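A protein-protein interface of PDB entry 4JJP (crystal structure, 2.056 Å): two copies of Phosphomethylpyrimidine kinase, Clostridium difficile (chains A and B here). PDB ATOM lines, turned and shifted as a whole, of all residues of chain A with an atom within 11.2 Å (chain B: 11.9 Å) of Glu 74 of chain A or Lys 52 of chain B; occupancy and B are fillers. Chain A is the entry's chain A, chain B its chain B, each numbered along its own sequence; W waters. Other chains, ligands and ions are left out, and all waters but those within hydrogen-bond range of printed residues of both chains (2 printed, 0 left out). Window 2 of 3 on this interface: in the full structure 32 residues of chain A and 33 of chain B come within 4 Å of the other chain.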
ATOM      1  N   PRO A  10     -23.658 -10.321  22.940  1.00  0.00           N
ATOM      2  CA  PRO A  10     -24.671  -9.808  22.035  1.00  0.00           C
ATOM      3  C   PRO A  10     -25.682 -10.839  21.516  1.00  0.00           C
ATOM      4  O   PRO A  10     -25.317 -11.991  21.240  1.00  0.00           O
ATOM      5  CB  PRO A  10     -23.858  -9.212  20.878  1.00  0.00           C
ATOM      6  CG  PRO A  10     -22.539  -9.827  20.955  1.00  0.00           C
ATOM      7  CD  PRO A  10     -22.328 -10.373  22.314  1.00  0.00           C
ATOM      8  N   LEU A  12     -29.161 -10.877  18.777  1.00  0.00           N
ATOM      9  CA  LEU A  12     -29.889 -10.130  17.757  1.00  0.00           C
ATOM     10  C   LEU A  12     -31.326 -10.600  17.609  1.00  0.00           C
ATOM     11  O   LEU A  12     -31.606 -11.806  17.717  1.00  0.00           O
ATOM     12  CB  LEU A  12     -29.206 -10.348  16.415  1.00  0.00           C
ATOM     13  CG  LEU A  12     -29.858  -9.790  15.154  1.00  0.00           C
ATOM     14  CD1 LEU A  12     -29.917  -8.253  15.277  1.00  0.00           C
ATOM     15  CD2 LEU A  12     -29.073 -10.280  13.927  1.00  0.00           C
ATOM     16  N   MET A  40     -29.492  -6.225  20.146  1.00  0.00           N
ATOM     17  CA  MET A  40     -29.344  -5.598  18.835  1.00  0.00           C
ATOM     18  C   MET A  40     -30.594  -5.973  18.024  1.00  0.00           C
ATOM     19  O   MET A  40     -31.248  -6.975  18.327  1.00  0.00           O
ATOM     20  CB  MET A  40     -28.132  -6.158  18.113  1.00  0.00           C
ATOM     21  CG  MET A  40     -26.820  -5.955  18.869  1.00  0.00           C
ATOM     22  SD  MET A  40     -25.405  -6.481  17.905  1.00  0.00           S
ATOM     23  CE  MET A  40     -25.513  -8.238  17.931  1.00  0.00           C
ATOM     24  N   VAL A  42     -32.536  -5.972  13.870  1.00  0.00           N
ATOM     25  CA  VAL A  42     -32.734  -5.614  12.489  1.00  0.00           C
ATOM     26  C   VAL A  42     -34.252  -5.451  12.387  1.00  0.00           C
ATOM     27  O   VAL A  42     -34.978  -6.411  12.552  1.00  0.00           O
ATOM     28  CB  VAL A  42     -32.297  -6.687  11.517  1.00  0.00           C
ATOM     29  CG1 VAL A  42     -32.835  -6.364  10.124  1.00  0.00           C
ATOM     30  CG2 VAL A  42     -30.766  -6.861  11.531  1.00  0.00           C
ATOM     31  N   ILE A  65     -32.926  -3.233   5.013  1.00  0.00           N
ATOM     32  CA  ILE A  65     -32.888  -4.473   5.814  1.00  0.00           C
ATOM     33  C   ILE A  65     -31.519  -5.163   5.623  1.00  0.00           C
ATOM     34  O   ILE A  65     -30.862  -5.603   6.586  1.00  0.00           O
ATOM     35  CB  ILE A  65     -34.090  -5.396   5.456  1.00  0.00           C
ATOM     36  CG1 ILE A  65     -35.369  -4.800   6.075  1.00  0.00           C
ATOM     37  CG2 ILE A  65     -33.875  -6.848   5.926  1.00  0.00           C
ATOM     38  CD1 ILE A  65     -36.673  -5.451   5.657  1.00  0.00           C
ATOM     39  N   LYS A  66     -31.085  -5.211   4.374  1.00  0.00           N
ATOM     40  CA  LYS A  66     -29.827  -5.829   4.045  1.00  0.00           C
ATOM     41  C   LYS A  66     -28.708  -5.129   4.779  1.00  0.00           C
ATOM     42  O   LYS A  66     -27.881  -5.792   5.385  1.00  0.00           O
ATOM     43  CB  LYS A  66     -29.590  -5.743   2.540  1.00  0.00           C
ATOM     44  CG  LYS A  66     -28.355  -6.432   2.064  1.00  0.00           C
ATOM     45  CD  LYS A  66     -28.344  -6.423   0.558  1.00  0.00           C
ATOM     46  CE  LYS A  66     -27.259  -7.298   0.037  1.00  0.00           C
ATOM     47  NZ  LYS A  66     -27.421  -7.488  -1.409  1.00  0.00           N
ATOM     48  N   LYS A  67     -28.693  -3.796   4.693  1.00  0.00           N
ATOM     49  CA  LYS A  67     -27.665  -2.957   5.327  1.00  0.00           C
ATOM     50  C   LYS A  67     -27.627  -3.118   6.842  1.00  0.00           C
ATOM     51  O   LYS A  67     -26.547  -3.117   7.430  1.00  0.00           O
ATOM     52  CB  LYS A  67     -27.840  -1.478   4.972  1.00  0.00           C
ATOM     53  CG  LYS A  67     -27.677  -1.165   3.464  1.00  0.00           C
ATOM     54  CD  LYS A  67     -26.384  -1.715   2.915  1.00  0.00           C
ATOM     55  CE  LYS A  67     -26.289  -1.528   1.427  1.00  0.00           C
ATOM     56  NZ  LYS A  67     -25.250  -2.457   0.902  1.00  0.00           N
ATOM     57  N   GLN A  68     -28.799  -3.241   7.465  1.00  0.00           N
ATOM     58  CA  GLN A  68     -28.870  -3.477   8.908  1.00  0.00           C
ATOM     59  C   GLN A  68     -28.223  -4.808   9.293  1.00  0.00           C
ATOM     60  O   GLN A  68     -27.484  -4.910  10.281  1.00  0.00           O
ATOM     61  CB  GLN A  68     -30.315  -3.505   9.369  1.00  0.00           C
ATOM     62  CG  GLN A  68     -30.980  -2.165   9.473  1.00  0.00           C
ATOM     63  CD  GLN A  68     -32.354  -2.297  10.016  1.00  0.00           C
ATOM     64  OE1 GLN A  68     -32.550  -2.267  11.248  1.00  0.00           O
ATOM     65  NE2 GLN A  68     -33.321  -2.529   9.136  1.00  0.00           N
ATOM     66  N   ILE A  69     -28.514  -5.827   8.497  1.00  0.00           N
ATOM     67  CA  ILE A  69     -27.964  -7.151   8.732  1.00  0.00           C
ATOM     68  C   ILE A  69     -26.429  -7.134   8.572  1.00  0.00           C
ATOM     69  O   ILE A  69     -25.691  -7.619   9.447  1.00  0.00           O
ATOM     70  CB  ILE A  69     -28.630  -8.196   7.804  1.00  0.00           C
ATOM     71  CG1 ILE A  69     -30.112  -8.332   8.177  1.00  0.00           C
ATOM     72  CG2 ILE A  69     -27.924  -9.565   7.915  1.00  0.00           C
ATOM     73  CD1 ILE A  69     -30.922  -9.206   7.255  1.00  0.00           C
ATOM     74  N   GLU A  70     -25.957  -6.568   7.461  1.00  0.00           N
ATOM     75  CA  GLU A  70     -24.526  -6.490   7.185  1.00  0.00           C
ATOM     76  C   GLU A  70     -23.815  -5.757   8.299  1.00  0.00           C
ATOM     77  O   GLU A  70     -22.755  -6.182   8.739  1.00  0.00           O
ATOM     78  CB  GLU A  70     -24.278  -5.786   5.864  1.00  0.00           C
ATOM     79  CG  GLU A  70     -24.756  -6.591   4.671  1.00  0.00           C
ATOM     80  CD  GLU A  70     -24.738  -5.807   3.344  1.00  0.00           C
ATOM     81  OE1 GLU A  70     -24.549  -4.566   3.358  1.00  0.00           O
ATOM     82  OE2 GLU A  70     -24.931  -6.458   2.291  1.00  0.00           O
ATOM     83  N   ALA A  71     -24.411  -4.653   8.751  1.00  0.00           N
ATOM     84  CA  ALA A  71     -23.827  -3.845   9.816  1.00  0.00           C
ATOM     85  C   ALA A  71     -23.605  -4.714  11.061  1.00  0.00           C
ATOM     86  O   ALA A  71     -22.519  -4.763  11.585  1.00  0.00           O
ATOM     87  CB  ALA A  71     -24.731  -2.605  10.134  1.00  0.00           C
ATOM     88  N   VAL A  72     -24.636  -5.433  11.489  1.00  0.00           N
ATOM     89  CA  VAL A  72     -24.552  -6.283  12.671  1.00  0.00           C
ATOM     90  C   VAL A  72     -23.524  -7.405  12.526  1.00  0.00           C
ATOM     91  O   VAL A  72     -22.667  -7.564  13.391  1.00  0.00           O
ATOM     92  CB  VAL A  72     -25.943  -6.857  13.041  1.00  0.00           C
ATOM     93  CG1 VAL A  72     -25.808  -7.972  14.070  1.00  0.00           C
ATOM     94  CG2 VAL A  72     -26.865  -5.732  13.526  1.00  0.00           C
ATOM     95  N   PHE A  73     -23.536  -8.129  11.415  1.00  0.00           N
ATOM     96  CA  PHE A  73     -22.597  -9.239  11.268  1.00  0.00           C
ATOM     97  C   PHE A  73     -21.128  -8.894  10.954  1.00  0.00           C
ATOM     98  O   PHE A  73     -20.228  -9.706  11.209  1.00  0.00           O
ATOM     99  CB  PHE A  73     -23.156 -10.286  10.294  1.00  0.00           C
ATOM    100  CG  PHE A  73     -24.297 -11.085  10.877  1.00  0.00           C
ATOM    101  CD1 PHE A  73     -24.043 -12.159  11.723  1.00  0.00           C
ATOM    102  CD2 PHE A  73     -25.614 -10.745  10.622  1.00  0.00           C
ATOM    103  CE1 PHE A  73     -25.081 -12.884  12.280  1.00  0.00           C
ATOM    104  CE2 PHE A  73     -26.655 -11.469  11.185  1.00  0.00           C
ATOM    105  CZ  PHE A  73     -26.381 -12.538  12.006  1.00  0.00           C
ATOM    106  N   GLU A  74     -20.878  -7.698  10.437  1.00  0.00           N
ATOM    107  CA  GLU A  74     -19.528  -7.305  10.048  1.00  0.00           C
ATOM    108  C   GLU A  74     -18.691  -6.702  11.183  1.00  0.00           C
ATOM    109  O   GLU A  74     -17.539  -6.333  10.961  1.00  0.00           O
ATOM    110  CB  GLU A  74     -19.585  -6.316   8.885  1.00  0.00           C
ATOM    111  CG  GLU A  74     -20.025  -6.913   7.553  1.00  0.00           C
ATOM    112  CD  GLU A  74     -20.027  -5.869   6.448  1.00  0.00           C
ATOM    113  OE1 GLU A  74     -19.983  -4.665   6.777  1.00  0.00           O
ATOM    114  OE2 GLU A  74     -20.052  -6.233   5.255  1.00  0.00           O
ATOM    115  N   ASP A  75     -19.265  -6.583  12.380  1.00  0.00           N
ATOM    116  CA  ASP A  75     -18.549  -6.028  13.532  1.00  0.00           C
ATOM    117  C   ASP A  75     -18.514  -7.169  14.551  1.00  0.00           C
ATOM    118  O   ASP A  75     -18.187  -8.288  14.159  1.00  0.00           O
ATOM    119  CB  ASP A  75     -19.273  -4.771  14.036  1.00  0.00           C
ATOM    120  CG  ASP A  75     -18.400  -3.890  14.932  1.00  0.00           C
ATOM    121  OD1 ASP A  75     -17.180  -4.154  15.081  1.00  0.00           O
ATOM    122  OD2 ASP A  75     -18.955  -2.908  15.479  1.00  0.00           O
ATOM    123  N   ILE A  76     -18.831  -6.951  15.828  1.00  0.00           N
ATOM    124  CA  ILE A  76     -18.826  -8.080  16.753  1.00  0.00           C
ATOM    125  C   ILE A  76     -20.190  -8.749  16.578  1.00  0.00           C
ATOM    126  O   ILE A  76     -21.218  -8.181  16.925  1.00  0.00           O
ATOM    127  CB  ILE A  76     -18.498  -7.680  18.213  1.00  0.00           C
ATOM    128  CG1 ILE A  76     -17.131  -6.979  18.276  1.00  0.00           C
ATOM    129  CG2 ILE A  76     -18.422  -8.915  19.084  1.00  0.00           C
ATOM    130  CD1 ILE A  76     -16.681  -6.548  19.704  1.00  0.00           C
ATOM    131  N   PRO A  77     -20.212  -9.955  16.004  1.00  0.00           N
ATOM    132  CA  PRO A  77     -21.514 -10.543  15.706  1.00  0.00           C
ATOM    133  C   PRO A  77     -22.280 -11.068  16.928  1.00  0.00           C
ATOM    134  O   PRO A  77     -21.698 -11.275  17.989  1.00  0.00           O
ATOM    135  CB  PRO A  77     -21.153 -11.698  14.774  1.00  0.00           C
ATOM    136  CG  PRO A  77     -19.811 -12.123  15.221  1.00  0.00           C
ATOM    137  CD  PRO A  77     -19.110 -10.863  15.647  1.00  0.00           C
ATOM    138  N   PRO A  78     -23.594 -11.279  16.769  1.00  0.00           N
ATOM    139  CA  PRO A  78     -24.388 -11.820  17.864  1.00  0.00           C
ATOM    140  C   PRO A  78     -24.044 -13.284  18.133  1.00  0.00           C
ATOM    141  O   PRO A  78     -23.689 -14.002  17.210  1.00  0.00           O
ATOM    142  CB  PRO A  78     -25.819 -11.721  17.323  1.00  0.00           C
ATOM    143  CG  PRO A  78     -25.661 -11.757  15.873  1.00  0.00           C
ATOM    144  CD  PRO A  78     -24.440 -10.949  15.611  1.00  0.00           C
ATOM    145  N   VAL A  81     -29.336 -15.597  17.563  1.00  0.00           N
ATOM    146  CA  VAL A  81     -30.210 -14.767  16.733  1.00  0.00           C
ATOM    147  C   VAL A  81     -31.655 -15.265  16.780  1.00  0.00           C
ATOM    148  O   VAL A  81     -31.913 -16.455  16.579  1.00  0.00           O
ATOM    149  CB  VAL A  81     -29.766 -14.801  15.219  1.00  0.00           C
ATOM    150  CG1 VAL A  81     -30.693 -13.925  14.368  1.00  0.00           C
ATOM    151  CG2 VAL A  81     -28.304 -14.370  15.061  1.00  0.00           C
ATOM    152  N   ASN A  98     -29.182 -13.619   3.660  1.00  0.00           N
ATOM    153  CA  ASN A  98     -28.205 -13.033   4.561  1.00  0.00           C
ATOM    154  C   ASN A  98     -27.799 -14.009   5.670  1.00  0.00           C
ATOM    155  O   ASN A  98     -26.624 -14.086   6.004  1.00  0.00           O
ATOM    156  CB  ASN A  98     -28.692 -11.674   5.107  1.00  0.00           C
ATOM    157  CG  ASN A  98     -28.532 -10.545   4.081  1.00  0.00           C
ATOM    158  OD1 ASN A  98     -27.434 -10.057   3.866  1.00  0.00           O
ATOM    159  ND2 ASN A  98     -29.620 -10.127   3.464  1.00  0.00           N
ATOM    160  N   LYS A 101     -25.223 -16.278   4.319  1.00  0.00           N
ATOM    161  CA  LYS A 101     -23.946 -15.597   4.196  1.00  0.00           C
ATOM    162  C   LYS A 101     -23.193 -15.549   5.546  1.00  0.00           C
ATOM    163  O   LYS A 101     -22.005 -15.782   5.597  1.00  0.00           O
ATOM    164  CB  LYS A 101     -24.202 -14.172   3.702  1.00  0.00           C
ATOM    165  CG  LYS A 101     -22.986 -13.351   3.357  1.00  0.00           C
ATOM    166  CD  LYS A 101     -23.439 -12.009   2.790  1.00  0.00           C
ATOM    167  CE  LYS A 101     -22.278 -11.111   2.481  1.00  0.00           C
ATOM    168  NZ  LYS A 101     -22.794  -9.757   2.132  1.00  0.00           N
ATOM    169  N   TYR A 102     -23.904 -15.258   6.628  1.00  0.00           N
ATOM    170  CA  TYR A 102     -23.294 -15.074   7.953  1.00  0.00           C
ATOM    171  C   TYR A 102     -23.252 -16.336   8.842  1.00  0.00           C
ATOM    172  O   TYR A 102     -22.463 -16.397   9.784  1.00  0.00           O
ATOM    173  CB  TYR A 102     -23.937 -13.858   8.632  1.00  0.00           C
ATOM    174  CG  TYR A 102     -23.697 -12.619   7.813  1.00  0.00           C
ATOM    175  CD1 TYR A 102     -22.402 -12.152   7.624  1.00  0.00           C
ATOM    176  CD2 TYR A 102     -24.740 -11.913   7.221  1.00  0.00           C
ATOM    177  CE1 TYR A 102     -22.143 -11.042   6.872  1.00  0.00           C
ATOM    178  CE2 TYR A 102     -24.486 -10.777   6.445  1.00  0.00           C
ATOM    179  CZ  TYR A 102     -23.183 -10.347   6.286  1.00  0.00           C
ATOM    180  OH  TYR A 102     -22.876  -9.230   5.547  1.00  0.00           O
ATOM    181  N   ASN A 103     -24.086 -17.326   8.498  1.00  0.00           N
ATOM    182  CA  ASN A 103     -24.156 -18.633   9.161  1.00  0.00           C
ATOM    183  C   ASN A 103     -24.076 -18.634  10.696  1.00  0.00           C
ATOM    184  O   ASN A 103     -23.160 -19.214  11.278  1.00  0.00           O
ATOM    185  CB  ASN A 103     -23.102 -19.574   8.563  1.00  0.00           C
ATOM    186  CG  ASN A 103     -23.441 -20.007   7.143  1.00  0.00           C
ATOM    187  OD1 ASN A 103     -24.587 -20.352   6.848  1.00  0.00           O
ATOM    188  ND2 ASN A 103     -22.446 -20.004   6.260  1.00  0.00           N
ATOM    189  N   PRO A 104     -25.043 -17.984  11.356  1.00  0.00           N
ATOM    190  CA  PRO A 104     -25.067 -17.993  12.829  1.00  0.00           C
ATOM    191  C   PRO A 104     -25.377 -19.406  13.402  1.00  0.00           C
ATOM    192  O   PRO A 104     -26.207 -20.151  12.859  1.00  0.00           O
ATOM    193  CB  PRO A 104     -26.169 -16.976  13.174  1.00  0.00           C
ATOM    194  CG  PRO A 104     -27.034 -16.931  11.988  1.00  0.00           C
ATOM    195  CD  PRO A 104     -26.144 -17.185  10.791  1.00  0.00           C
ATOM    196  N   ASP B  18     -31.160   2.263  15.759  1.00  0.00           N
ATOM    197  CA  ASP B  18     -29.748   1.935  15.575  1.00  0.00           C
ATOM    198  C   ASP B  18     -29.552   0.417  15.668  1.00  0.00           C
ATOM    199  O   ASP B  18     -29.706  -0.172  16.744  1.00  0.00           O
ATOM    200  CB  ASP B  18     -28.897   2.662  16.639  1.00  0.00           C
ATOM    201  CG  ASP B  18     -27.448   2.123  16.756  1.00  0.00           C
ATOM    202  OD1 ASP B  18     -26.892   1.516  15.798  1.00  0.00           O
ATOM    203  OD2 ASP B  18     -26.848   2.326  17.848  1.00  0.00           O
ATOM    204  N   SER B  19     -29.177  -0.195  14.542  1.00  0.00           N
ATOM    205  CA  SER B  19     -28.984  -1.632  14.455  1.00  0.00           C
ATOM    206  C   SER B  19     -27.938  -2.174  15.446  1.00  0.00           C
ATOM    207  O   SER B  19     -28.095  -3.282  15.940  1.00  0.00           O
ATOM    208  CB  SER B  19     -28.663  -2.060  13.011  1.00  0.00           C
ATOM    209  OG  SER B  19     -27.466  -1.489  12.522  1.00  0.00           O
ATOM    210  N   SER B  20     -26.917  -1.395  15.781  1.00  0.00           N
ATOM    211  CA  SER B  20     -25.888  -1.867  16.717  1.00  0.00           C
ATOM    212  C   SER B  20     -26.384  -2.000  18.153  1.00  0.00           C
ATOM    213  O   SER B  20     -25.734  -2.629  18.953  1.00  0.00           O
ATOM    214  CB  SER B  20     -24.708  -0.902  16.756  1.00  0.00           C
ATOM    215  OG  SER B  20     -25.042   0.313  17.437  1.00  0.00           O
ATOM    216  N   GLY B  21     -27.485  -1.342  18.486  1.00  0.00           N
ATOM    217  CA  GLY B  21     -28.028  -1.374  19.837  1.00  0.00           C
ATOM    218  C   GLY B  21     -27.293  -0.464  20.824  1.00  0.00           C
ATOM    219  O   GLY B  21     -27.599  -0.495  22.026  1.00  0.00           O
ATOM    220  N   GLY B  22     -26.336   0.339  20.343  1.00  0.00           N
ATOM    221  CA  GLY B  22     -25.571   1.270  21.202  1.00  0.00           C
ATOM    222  C   GLY B  22     -26.261   2.609  21.493  1.00  0.00           C
ATOM    223  O   GLY B  22     -25.996   3.242  22.527  1.00  0.00           O
ATOM    224  N   ALA B  48     -28.467   1.819   9.725  1.00  0.00           N
ATOM    225  CA  ALA B  48     -27.633   0.634   9.692  1.00  0.00           C
ATOM    226  C   ALA B  48     -26.242   1.154  10.043  1.00  0.00           C
ATOM    227  O   ALA B  48     -25.637   1.894   9.254  1.00  0.00           O
ATOM    228  CB  ALA B  48     -27.632  -0.019   8.305  1.00  0.00           C
ATOM    229  N   GLN B  49     -25.752   0.796  11.230  1.00  0.00           N
ATOM    230  CA  GLN B  49     -24.415   1.190  11.639  1.00  0.00           C
ATOM    231  C   GLN B  49     -23.783   0.260  12.685  1.00  0.00           C
ATOM    232  O   GLN B  49     -24.483  -0.477  13.378  1.00  0.00           O
ATOM    233  CB  GLN B  49     -24.446   2.612  12.176  1.00  0.00           C
ATOM    234  CG  GLN B  49     -25.273   2.766  13.405  1.00  0.00           C
ATOM    235  CD  GLN B  49     -25.162   4.143  13.999  1.00  0.00           C
ATOM    236  OE1 GLN B  49     -24.402   4.982  13.520  1.00  0.00           O
ATOM    237  NE2 GLN B  49     -25.915   4.382  15.056  1.00  0.00           N
ATOM    238  N   ASN B  50     -22.454   0.294  12.771  1.00  0.00           N
ATOM    239  CA  ASN B  50     -21.696  -0.480  13.772  1.00  0.00           C
ATOM    240  C   ASN B  50     -20.492   0.348  14.192  1.00  0.00           C
ATOM    241  O   ASN B  50     -20.322   1.459  13.695  1.00  0.00           O
ATOM    242  CB  ASN B  50     -21.298  -1.869  13.244  1.00  0.00           C
ATOM    243  CG  ASN B  50     -20.409  -1.814  12.021  1.00  0.00           C
ATOM    244  OD1 ASN B  50     -19.771  -0.807  11.751  1.00  0.00           O
ATOM    245  ND2 ASN B  50     -20.348  -2.913  11.281  1.00  0.00           N
ATOM    246  N   THR B  51     -19.650  -0.181  15.080  1.00  0.00           N
ATOM    247  CA  THR B  51     -18.465   0.571  15.571  1.00  0.00           C
ATOM    248  C   THR B  51     -17.502   1.070  14.464  1.00  0.00           C
ATOM    249  O   THR B  51     -16.682   1.945  14.709  1.00  0.00           O
ATOM    250  CB  THR B  51     -17.614  -0.248  16.614  1.00  0.00           C
ATOM    251  OG1 THR B  51     -16.901  -1.299  15.952  1.00  0.00           O
ATOM    252  CG2 THR B  51     -18.475  -0.826  17.711  1.00  0.00           C
ATOM    253  N   LYS B  52     -17.595   0.511  13.261  1.00  0.00           N
ATOM    254  CA  LYS B  52     -16.735   0.904  12.152  1.00  0.00           C
ATOM    255  C   LYS B  52     -17.305   1.998  11.224  1.00  0.00           C
ATOM    256  O   LYS B  52     -16.573   2.541  10.394  1.00  0.00           O
ATOM    257  CB  LYS B  52     -16.359  -0.338  11.338  1.00  0.00           C
ATOM    258  CG  LYS B  52     -15.710  -1.447  12.182  1.00  0.00           C
ATOM    259  CD  LYS B  52     -15.094  -2.554  11.331  1.00  0.00           C
ATOM    260  CE  LYS B  52     -16.142  -3.339  10.540  1.00  0.00           C
ATOM    261  NZ  LYS B  52     -15.507  -4.421   9.721  1.00  0.00           N
ATOM    262  N   GLY B  53     -18.590   2.326  11.347  1.00  0.00           N
ATOM    263  CA  GLY B  53     -19.195   3.360  10.498  1.00  0.00           C
ATOM    264  C   GLY B  53     -20.667   3.184  10.166  1.00  0.00           C
ATOM    265  O   GLY B  53     -21.236   2.104  10.372  1.00  0.00           O
ATOM    266  N   VAL B  54     -21.286   4.256   9.666  1.00  0.00           N
ATOM    267  CA  VAL B  54     -22.693   4.221   9.264  1.00  0.00           C
ATOM    268  C   VAL B  54     -22.788   3.732   7.814  1.00  0.00           C
ATOM    269  O   VAL B  54     -22.098   4.238   6.914  1.00  0.00           O
ATOM    270  CB  VAL B  54     -23.417   5.576   9.452  1.00  0.00           C
ATOM    271  CG1 VAL B  54     -23.149   6.115  10.845  1.00  0.00           C
ATOM    272  CG2 VAL B  54     -22.991   6.566   8.428  1.00  0.00           C
ATOM    273  N   PHE B  55     -23.617   2.708   7.618  1.00  0.00           N
ATOM    274  CA  PHE B  55     -23.832   2.101   6.314  1.00  0.00           C
ATOM    275  C   PHE B  55     -25.043   2.743   5.647  1.00  0.00           C
ATOM    276  O   PHE B  55     -25.123   2.746   4.431  1.00  0.00           O
ATOM    277  CB  PHE B  55     -24.103   0.598   6.433  1.00  0.00           C
ATOM    278  CG  PHE B  55     -22.927  -0.221   6.899  1.00  0.00           C
ATOM    279  CD1 PHE B  55     -22.371  -0.031   8.166  1.00  0.00           C
ATOM    280  CD2 PHE B  55     -22.420  -1.237   6.091  1.00  0.00           C
ATOM    281  CE1 PHE B  55     -21.303  -0.810   8.601  1.00  0.00           C
ATOM    282  CE2 PHE B  55     -21.351  -2.025   6.515  1.00  0.00           C
ATOM    283  CZ  PHE B  55     -20.787  -1.813   7.774  1.00  0.00           C
ATOM    284  N   ALA B  56     -25.986   3.271   6.430  1.00  0.00           N
ATOM    285  CA  ALA B  56     -27.189   3.867   5.842  1.00  0.00           C
ATOM    286  C   ALA B  56     -28.088   4.455   6.900  1.00  0.00           C
ATOM    287  O   ALA B  56     -28.241   3.859   7.962  1.00  0.00           O
ATOM    288  CB  ALA B  56     -27.971   2.821   5.053  1.00  0.00           C
ATOM    289  N   ILE B 114     -24.293  14.097  17.082  1.00  0.00           N
ATOM    290  CA  ILE B 114     -23.136  13.309  16.664  1.00  0.00           C
ATOM    291  C   ILE B 114     -23.544  11.829  16.742  1.00  0.00           C
ATOM    292  O   ILE B 114     -22.888  10.951  16.168  1.00  0.00           O
ATOM    293  CB  ILE B 114     -21.880  13.581  17.587  1.00  0.00           C
ATOM    294  CG1 ILE B 114     -21.788  15.050  18.025  1.00  0.00           C
ATOM    295  CG2 ILE B 114     -20.581  13.161  16.897  1.00  0.00           C
ATOM    296  CD1 ILE B 114     -20.558  15.336  18.840  1.00  0.00           C
HETATM  297  O   HOH W   1     -24.817  -2.854  13.774  1.00  0.00           O
HETATM  298  O   HOH W   2     -31.999  -0.033  12.580  1.00  0.00           O
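Hydrophobic or aromatic side chains of chain B within 4 Å of the printed part of chain A: Ala 48 and Phe 55. Of the 24 printed residues of chain A, 7 touch a printed residue of chain B. Hydrophobic or aromatic side chains of chain A that line the printed part of chain B: Met 40, Ala 71 and Val 72. Among the printed residues, 12 pairs touch across the chains. Among the printed residues, no Asp or Glu carboxylate lies within 4 Å of a Lys or Arg side-chain nitrogen of the other chain.
O of Ser 19 of chain B touches CB of Met 40 of chain A, at 3.6 Å. O of Ser 20 of chain B touches CG of Met 40 of chain A, at 3.5 Å. Lys 67 of chain A touches Ala 48 of chain B. N of Gln 68 of chain A touches CB of Ala 48 of chain B, at 3.5 Å. Ala 71 of chain A touches Ser 19 of chain B. N of Gln 49 of chain B touches CB of Ala 71 of chain A (3.7 Å). Val 72 of chain A touches Ser 19 of chain B. OE1 of Glu 74 of chain A touches CE2 of Phe 55 of chain B, at 3.0 Å. CB of Asn 50 of chain B touches OD2 of Asp 75 of chain A (3.4 Å).
Water W1 lies within hydrogen-bond range of the backbone carbonyl oxygen of Gln 49 of chain B (2.4 Å), the side-chain hydroxyl of Ser 19 of chain B (3.2 Å), the backbone NH of Ser 20 of chain B (3.3 Å) and the backbone NH of Val 72 of chain A (3.5 Å). Water W2 bridges the side-chain amide oxygen (OE1) of Gln 68 of chain A (2.7 Å) and the backbone NH (N) of Ser 19 of chain B (3.4 Å).
No position is printed for both chains. Of the 12 pairs that touch across the chains among the printed residues, none has its exchanged pair printed and touching as well.
Val 42 of chain A touches none of the printed residues of chain B. Printed residues of chain B within 4 Å of Lys 67 of chain A: Ala 48 (3.4 Å). Of the printed residues of chain B, Gln 68 of chain A touches Ala 48. No residue of chain B comes within 4 Å of Glu 70 of chain A. Val 72 of chain A touches one residue of chain B. Of chain B, only Lys 52 and Phe 55 come within 4 Å of Glu 74 of chain A. Of chain B, only Asn 50 (3.4 Å) and Thr 51 (2.7 Å) come within 4 Å of Asp 75 of chain A. Of chain A, only Ala 71 (2.9 Å) and Asp 75 (3.4 Å) come within 4 Å of Asn 50 of chain B. Of chain A, only Asp 75 (2.7 Å) comes within 4 Å of Thr 51 of chain B. Of chain A, only Glu 74 (3.1 Å) comes within 4 Å of Lys 52 of chain B. No residue of chain A comes within 4 Å of Gly 53 of chain B. The nearest residue of chain B that does not touch Glu 74 of chain A is Asn 50 of chain B (4.1 Å). The nearest residue of chain A that does not touch Lys 52 of chain B is Asp 75 of chain A (4.2 Å). The nearest printed residue of chain B that does not touch Gln 68 of chain A is Ser 19 of chain B (4.1 Å).
The side-chain carboxylate of Asp 18 of chain B lies within hydrogen-bond range of the side-chain amide nitrogen of Gln 49 of chain B (3.1 Å). The backbone carbonyl oxygen (O) of Ala 48 of chain B sits at hydrogen-bond distance from the backbone NH (N) of Phe 55 of chain B (2.7 Å). N of Ala 48 of chain B lies within hydrogen-bond range of O of Ala 56 of chain B, at 2.7 Å. The side-chain amide oxygen (OD1) of Asn 50 of chain B lies within hydrogen-bond range of the backbone NH (N) of Lys 52 of chain B (3.0 Å). N of Gly 53 of chain B sits at hydrogen-bond distance from OD1 of Asn 50 of chain B, at 3.4 Å.
The backbone carbonyl oxygen (O) of Ala 71 of chain A sits at hydrogen-bond distance from the side-chain amide nitrogen (ND2) of Asn 50 of chain B (2.9 Å). The side-chain amino group (NZ) of Lys 52 of chain B sits at hydrogen-bond distance from the backbone carbonyl oxygen (O) of Glu 74 of chain A, 3.1 Å away. The side-chain hydroxyl of Thr 51 of chain B is in hydrogen-bond range of the side-chain carboxylate of Asp 75 of chain A (2.7 Å).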
